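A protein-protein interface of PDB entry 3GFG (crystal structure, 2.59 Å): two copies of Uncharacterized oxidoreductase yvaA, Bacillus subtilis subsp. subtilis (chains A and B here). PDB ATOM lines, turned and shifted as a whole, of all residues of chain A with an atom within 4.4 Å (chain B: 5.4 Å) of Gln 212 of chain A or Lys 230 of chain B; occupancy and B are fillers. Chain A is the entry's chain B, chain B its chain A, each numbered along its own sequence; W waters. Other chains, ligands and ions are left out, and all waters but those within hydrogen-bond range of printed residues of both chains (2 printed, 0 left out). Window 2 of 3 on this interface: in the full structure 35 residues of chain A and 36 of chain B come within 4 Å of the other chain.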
ATOM      1  N   MET A 210     -29.763   7.245 -32.130  1.00  0.00           N
ATOM      2  CA  MET A 210     -29.356   6.302 -31.092  1.00  0.00           C
ATOM      3  C   MET A 210     -30.454   6.001 -30.065  1.00  0.00           C
ATOM      4  O   MET A 210     -31.492   6.644 -30.030  1.00  0.00           O
ATOM      5  CB  MET A 210     -28.075   6.793 -30.392  1.00  0.00           C
ATOM      6  CG  MET A 210     -28.237   8.099 -29.621  1.00  0.00           C
ATOM      7  SD  MET A 210     -26.898   8.554 -28.478  1.00  0.00           S
ATOM      8  CE  MET A 210     -25.429   8.476 -29.482  1.00  0.00           C
ATOM      9  N   ALA A 211     -30.212   4.988 -29.249  1.00  0.00           N
ATOM     10  CA  ALA A 211     -31.027   4.731 -28.084  1.00  0.00           C
ATOM     11  C   ALA A 211     -30.224   5.162 -26.839  1.00  0.00           C
ATOM     12  O   ALA A 211     -29.249   4.514 -26.479  1.00  0.00           O
ATOM     13  CB  ALA A 211     -31.384   3.241 -28.017  1.00  0.00           C
ATOM     14  N   GLN A 212     -30.632   6.257 -26.201  1.00  0.00           N
ATOM     15  CA  GLN A 212     -30.003   6.741 -24.956  1.00  0.00           C
ATOM     16  C   GLN A 212     -30.462   6.002 -23.711  1.00  0.00           C
ATOM     17  O   GLN A 212     -29.743   5.976 -22.732  1.00  0.00           O
ATOM     18  CB  GLN A 212     -30.323   8.217 -24.725  1.00  0.00           C
ATOM     19  CG  GLN A 212     -29.242   9.219 -25.021  1.00  0.00           C
ATOM     20  CD  GLN A 212     -29.760  10.644 -24.839  1.00  0.00           C
ATOM     21  OE1 GLN A 212     -30.968  10.896 -24.910  1.00  0.00           O
ATOM     22  NE2 GLN A 212     -28.851  11.579 -24.618  1.00  0.00           N
ATOM     23  N   ARG A 213     -31.679   5.470 -23.713  1.00  0.00           N
ATOM     24  CA  ARG A 213     -32.210   4.845 -22.508  1.00  0.00           C
ATOM     25  C   ARG A 213     -31.541   3.522 -22.196  1.00  0.00           C
ATOM     26  O   ARG A 213     -31.251   2.722 -23.088  1.00  0.00           O
ATOM     27  CB  ARG A 213     -33.716   4.647 -22.589  1.00  0.00           C
ATOM     28  CG  ARG A 213     -34.475   5.907 -22.352  1.00  0.00           C
ATOM     29  CD  ARG A 213     -35.885   5.791 -22.819  1.00  0.00           C
ATOM     30  NE  ARG A 213     -35.984   4.916 -23.962  1.00  0.00           N
ATOM     31  CZ  ARG A 213     -37.121   4.614 -24.572  1.00  0.00           C
ATOM     32  NH1 ARG A 213     -38.265   5.147 -24.137  1.00  0.00           N
ATOM     33  NH2 ARG A 213     -37.109   3.784 -25.618  1.00  0.00           N
ATOM     34  N   GLU A 214     -31.300   3.307 -20.909  1.00  0.00           N
ATOM     35  CA  GLU A 214     -30.701   2.081 -20.457  1.00  0.00           C
ATOM     36  C   GLU A 214     -31.592   0.930 -20.950  1.00  0.00           C
ATOM     37  O   GLU A 214     -32.835   0.997 -20.849  1.00  0.00           O
ATOM     38  CB  GLU A 214     -30.582   2.103 -18.939  1.00  0.00           C
ATOM     39  CG  GLU A 214     -29.271   1.537 -18.432  1.00  0.00           C
ATOM     40  CD  GLU A 214     -29.474   0.628 -17.220  1.00  0.00           C
ATOM     41  OE1 GLU A 214     -30.633   0.540 -16.736  1.00  0.00           O
ATOM     42  OE2 GLU A 214     -28.488   0.003 -16.750  1.00  0.00           O
ATOM     43  N   ASP A 220     -34.523   6.380 -29.573  1.00  0.00           N
ATOM     44  CA  ASP A 220     -35.172   7.289 -28.633  1.00  0.00           C
ATOM     45  C   ASP A 220     -34.519   8.664 -28.652  1.00  0.00           C
ATOM     46  O   ASP A 220     -34.959   9.574 -27.940  1.00  0.00           O
ATOM     47  CB  ASP A 220     -35.244   6.690 -27.207  1.00  0.00           C
ATOM     48  CG  ASP A 220     -33.874   6.514 -26.552  1.00  0.00           C
ATOM     49  OD1 ASP A 220     -32.976   7.369 -26.741  1.00  0.00           O
ATOM     50  OD2 ASP A 220     -33.699   5.542 -25.781  1.00  0.00           O
ATOM     51  N   TYR A 221     -33.484   8.795 -29.483  1.00  0.00           N
ATOM     52  CA  TYR A 221     -32.756  10.050 -29.642  1.00  0.00           C
ATOM     53  C   TYR A 221     -32.352  10.297 -31.097  1.00  0.00           C
ATOM     54  O   TYR A 221     -31.837   9.403 -31.814  1.00  0.00           O
ATOM     55  CB  TYR A 221     -31.512  10.083 -28.722  1.00  0.00           C
ATOM     56  CG  TYR A 221     -30.586  11.271 -28.925  1.00  0.00           C
ATOM     57  CD1 TYR A 221     -30.648  12.384 -28.071  1.00  0.00           C
ATOM     58  CD2 TYR A 221     -29.651  11.297 -29.976  1.00  0.00           C
ATOM     59  CE1 TYR A 221     -29.808  13.490 -28.256  1.00  0.00           C
ATOM     60  CE2 TYR A 221     -28.820  12.387 -30.164  1.00  0.00           C
ATOM     61  CZ  TYR A 221     -28.898  13.478 -29.298  1.00  0.00           C
ATOM     62  OH  TYR A 221     -28.067  14.564 -29.472  1.00  0.00           O
ATOM     63  N   ILE A 240     -35.148  11.533 -22.586  1.00  0.00           N
ATOM     64  CA  ILE A 240     -34.828  11.773 -21.182  1.00  0.00           C
ATOM     65  C   ILE A 240     -34.665  13.283 -20.891  1.00  0.00           C
ATOM     66  O   ILE A 240     -33.622  13.727 -20.390  1.00  0.00           O
ATOM     67  CB  ILE A 240     -33.559  11.020 -20.723  1.00  0.00           C
ATOM     68  CG1 ILE A 240     -33.351   9.709 -21.511  1.00  0.00           C
ATOM     69  CG2 ILE A 240     -33.606  10.779 -19.203  1.00  0.00           C
ATOM     70  CD1 ILE A 240     -32.394   8.673 -20.815  1.00  0.00           C
ATOM     71  N   ASP B 154     -26.441  12.350 -13.696  1.00  0.00           N
ATOM     72  CA  ASP B 154     -26.436  11.563 -14.935  1.00  0.00           C
ATOM     73  C   ASP B 154     -26.809  12.360 -16.177  1.00  0.00           C
ATOM     74  O   ASP B 154     -27.770  12.027 -16.896  1.00  0.00           O
ATOM     75  CB  ASP B 154     -27.345  10.335 -14.820  1.00  0.00           C
ATOM     76  CG  ASP B 154     -27.039   9.492 -13.613  1.00  0.00           C
ATOM     77  OD1 ASP B 154     -26.043   8.725 -13.630  1.00  0.00           O
ATOM     78  OD2 ASP B 154     -27.810   9.575 -12.629  1.00  0.00           O
ATOM     79  N   ASN B 156     -27.332  13.434 -19.655  1.00  0.00           N
ATOM     80  CA  ASN B 156     -27.363  12.857 -20.983  1.00  0.00           C
ATOM     81  C   ASN B 156     -27.245  13.889 -22.130  1.00  0.00           C
ATOM     82  O   ASN B 156     -26.760  13.549 -23.185  1.00  0.00           O
ATOM     83  CB  ASN B 156     -28.618  11.989 -21.151  1.00  0.00           C
ATOM     84  CG  ASN B 156     -29.909  12.775 -20.980  1.00  0.00           C
ATOM     85  OD1 ASN B 156     -30.333  13.486 -21.883  1.00  0.00           O
ATOM     86  ND2 ASN B 156     -30.554  12.629 -19.832  1.00  0.00           N
ATOM     87  N   THR B 157     -27.682  15.131 -21.929  1.00  0.00           N
ATOM     88  CA  THR B 157     -27.627  16.149 -22.989  1.00  0.00           C
ATOM     89  C   THR B 157     -27.145  17.486 -22.445  1.00  0.00           C
ATOM     90  O   THR B 157     -27.671  17.983 -21.456  1.00  0.00           O
ATOM     91  CB  THR B 157     -29.008  16.318 -23.709  1.00  0.00           C
ATOM     92  OG1 THR B 157     -29.538  15.026 -24.039  1.00  0.00           O
ATOM     93  CG2 THR B 157     -28.882  17.120 -25.021  1.00  0.00           C
ATOM     94  N   TYR B 228     -19.964  11.474 -26.208  1.00  0.00           N
ATOM     95  CA  TYR B 228     -19.508  10.826 -24.974  1.00  0.00           C
ATOM     96  C   TYR B 228     -20.250   9.509 -24.725  1.00  0.00           C
ATOM     97  O   TYR B 228     -20.220   8.999 -23.613  1.00  0.00           O
ATOM     98  CB  TYR B 228     -19.735  11.737 -23.757  1.00  0.00           C
ATOM     99  CG  TYR B 228     -18.855  12.963 -23.709  1.00  0.00           C
ATOM    100  CD1 TYR B 228     -17.591  12.908 -23.126  1.00  0.00           C
ATOM    101  CD2 TYR B 228     -19.292  14.180 -24.249  1.00  0.00           C
ATOM    102  CE1 TYR B 228     -16.775  14.019 -23.088  1.00  0.00           C
ATOM    103  CE2 TYR B 228     -18.481  15.313 -24.223  1.00  0.00           C
ATOM    104  CZ  TYR B 228     -17.222  15.224 -23.647  1.00  0.00           C
ATOM    105  OH  TYR B 228     -16.413  16.329 -23.610  1.00  0.00           O
ATOM    106  N   GLY B 229     -20.927   8.974 -25.746  1.00  0.00           N
ATOM    107  CA  GLY B 229     -21.721   7.751 -25.600  1.00  0.00           C
ATOM    108  C   GLY B 229     -23.185   8.115 -25.440  1.00  0.00           C
ATOM    109  O   GLY B 229     -23.805   8.698 -26.341  1.00  0.00           O
ATOM    110  N   LYS B 230     -23.726   7.756 -24.281  1.00  0.00           N
ATOM    111  CA  LYS B 230     -25.056   8.150 -23.840  1.00  0.00           C
ATOM    112  C   LYS B 230     -25.147   9.681 -23.759  1.00  0.00           C
ATOM    113  O   LYS B 230     -26.146  10.282 -24.156  1.00  0.00           O
ATOM    114  CB  LYS B 230     -25.336   7.500 -22.476  1.00  0.00           C
ATOM    115  CG  LYS B 230     -26.621   7.937 -21.789  1.00  0.00           C
ATOM    116  CD  LYS B 230     -26.539   7.680 -20.257  1.00  0.00           C
ATOM    117  CE  LYS B 230     -27.915   7.781 -19.538  1.00  0.00           C
ATOM    118  NZ  LYS B 230     -28.925   6.762 -20.006  1.00  0.00           N
ATOM    119  N   LEU B 231     -24.083  10.308 -23.277  1.00  0.00           N
ATOM    120  CA  LEU B 231     -24.025  11.759 -23.202  1.00  0.00           C
ATOM    121  C   LEU B 231     -23.612  12.420 -24.551  1.00  0.00           C
ATOM    122  O   LEU B 231     -22.641  12.006 -25.183  1.00  0.00           O
ATOM    123  CB  LEU B 231     -23.117  12.176 -22.040  1.00  0.00           C
ATOM    124  CG  LEU B 231     -22.583  13.600 -22.031  1.00  0.00           C
ATOM    125  CD1 LEU B 231     -23.706  14.645 -21.802  1.00  0.00           C
ATOM    126  CD2 LEU B 231     -21.467  13.667 -20.973  1.00  0.00           C
ATOM    127  N   GLN B 232     -24.388  13.427 -24.975  1.00  0.00           N
ATOM    128  CA  GLN B 232     -24.138  14.204 -26.186  1.00  0.00           C
ATOM    129  C   GLN B 232     -23.994  15.674 -25.812  1.00  0.00           C
ATOM    130  O   GLN B 232     -24.927  16.260 -25.238  1.00  0.00           O
ATOM    131  CB  GLN B 232     -25.300  14.081 -27.184  1.00  0.00           C
ATOM    132  CG  GLN B 232     -25.504  12.734 -27.821  1.00  0.00           C
ATOM    133  CD  GLN B 232     -24.344  12.293 -28.728  1.00  0.00           C
ATOM    134  OE1 GLN B 232     -24.133  12.866 -29.800  1.00  0.00           O
ATOM    135  NE2 GLN B 232     -23.610  11.258 -28.308  1.00  0.00           N
HETATM  136  O   HOH W   1     -32.460  12.917 -23.678  1.00  0.00           O
HETATM  137  O   HOH W   2     -26.033  13.937 -31.099  1.00  0.00           O
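Of the 8 printed residues of chain A, 4 touch a printed residue of chain B.
Hydrophobic or aromatic side chains of chain A within 4 Å of the printed part of chain B: Met 210, Tyr 221 and Ile 240.
Among the printed residues, 7 pairs touch across the chains.
Among the printed residues, no Asp or Glu carboxylate lies within 4 Å of a Lys or Arg side-chain nitrogen of the other chain.
Water W2 lies within hydrogen-bond range of the side-chain amide oxygen (OE1) of Gln 232 of chain B and the side-chain hydroxyl (OH) of Tyr 221 of chain A.
Water W1 lies within hydrogen-bond range of the side-chain amide oxygen (OE1) of Gln 212 of chain A (2.8 Å), the side-chain amide oxygen (OD1) of Asn 156 of chain B (2.8 Å) and the backbone NH (N) of Ile 240 of chain A (3.2 Å).
Among the printed residues, pairs that only touch across the chains: Met 210 of chain A with Gln 232 of chain B (3.5 Å), Gln 212 of chain A with Thr 157 of chain B (3.6 Å) and Tyr 221 of chain A with Gln 232 of chain B (3.6 Å).
Ala 211 of chain A touches none of the printed residues of chain B.
Glu 214 of chain A touches none of the printed residues of chain B.
Printed residues of chain B within 4 Å of Tyr 221 of chain A: Gln 232 (3.6 Å).
Of the printed residues of chain A, Thr 157 of chain B touches Gln 212 (3.6 Å).
The nearest residue of chain B that does not touch Gln 212 of chain A is Gln 232 of chain B (4.8 Å).
The nearest residue of chain A that does not touch Lys 230 of chain B is Ile 240 of chain A (4.04 Å).
The nearest printed residue of chain A that does not touch Asn 156 of chain B is Tyr 221 of chain A (5.9 Å).
No position is printed for both chains.
Of the 7 pairs that touch across the chains among the printed residues, none has its exchanged pair printed and touching as well.
N of Gln 212 of chain A lies within hydrogen-bond range of OD1 of Asp 220 of chain A (2.6 Å).
The backbone carbonyl oxygen (O) of Asn 156 of chain B sits at hydrogen-bond distance from the backbone NH (N) of Gln 232 of chain B, 3.0 Å away.
The side-chain amide nitrogen of Gln 232 of chain B sits at hydrogen-bond distance from the backbone carbonyl oxygen of Gly 229 of chain B.
OG1 of Thr 157 of chain B sits at hydrogen-bond distance from OD1 of Asn 156 of chain B (2.8 Å).
The backbone carbonyl oxygen (O) of Met 210 of chain A is in hydrogen-bond range of the backbone NH (N) of Asp 220 of chain A, at 3.1 Å.
The backbone carbonyl oxygen of Met 210 of chain A lies within hydrogen-bond range of the backbone NH of Tyr 221 of chain A, 3.0 Å away.
The side-chain amide nitrogen (ND2) of Asn 156 of chain B lies within hydrogen-bond range of the backbone carbonyl oxygen (O) of Ile 240 of chain A (3.3 Å).
The backbone carbonyl oxygen (O) of Gly 229 of chain B sits close to the side-chain sulfur (SD) of Met 210 of chain A (3.8 Å).
NZ of Lys 230 of chain B is in hydrogen-bond range of O of Gln 212 of chain A (3.0 Å).
O of Asn 156 of chain B lies within hydrogen-bond range of NE2 of Gln 212 of chain A (3.2 Å).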
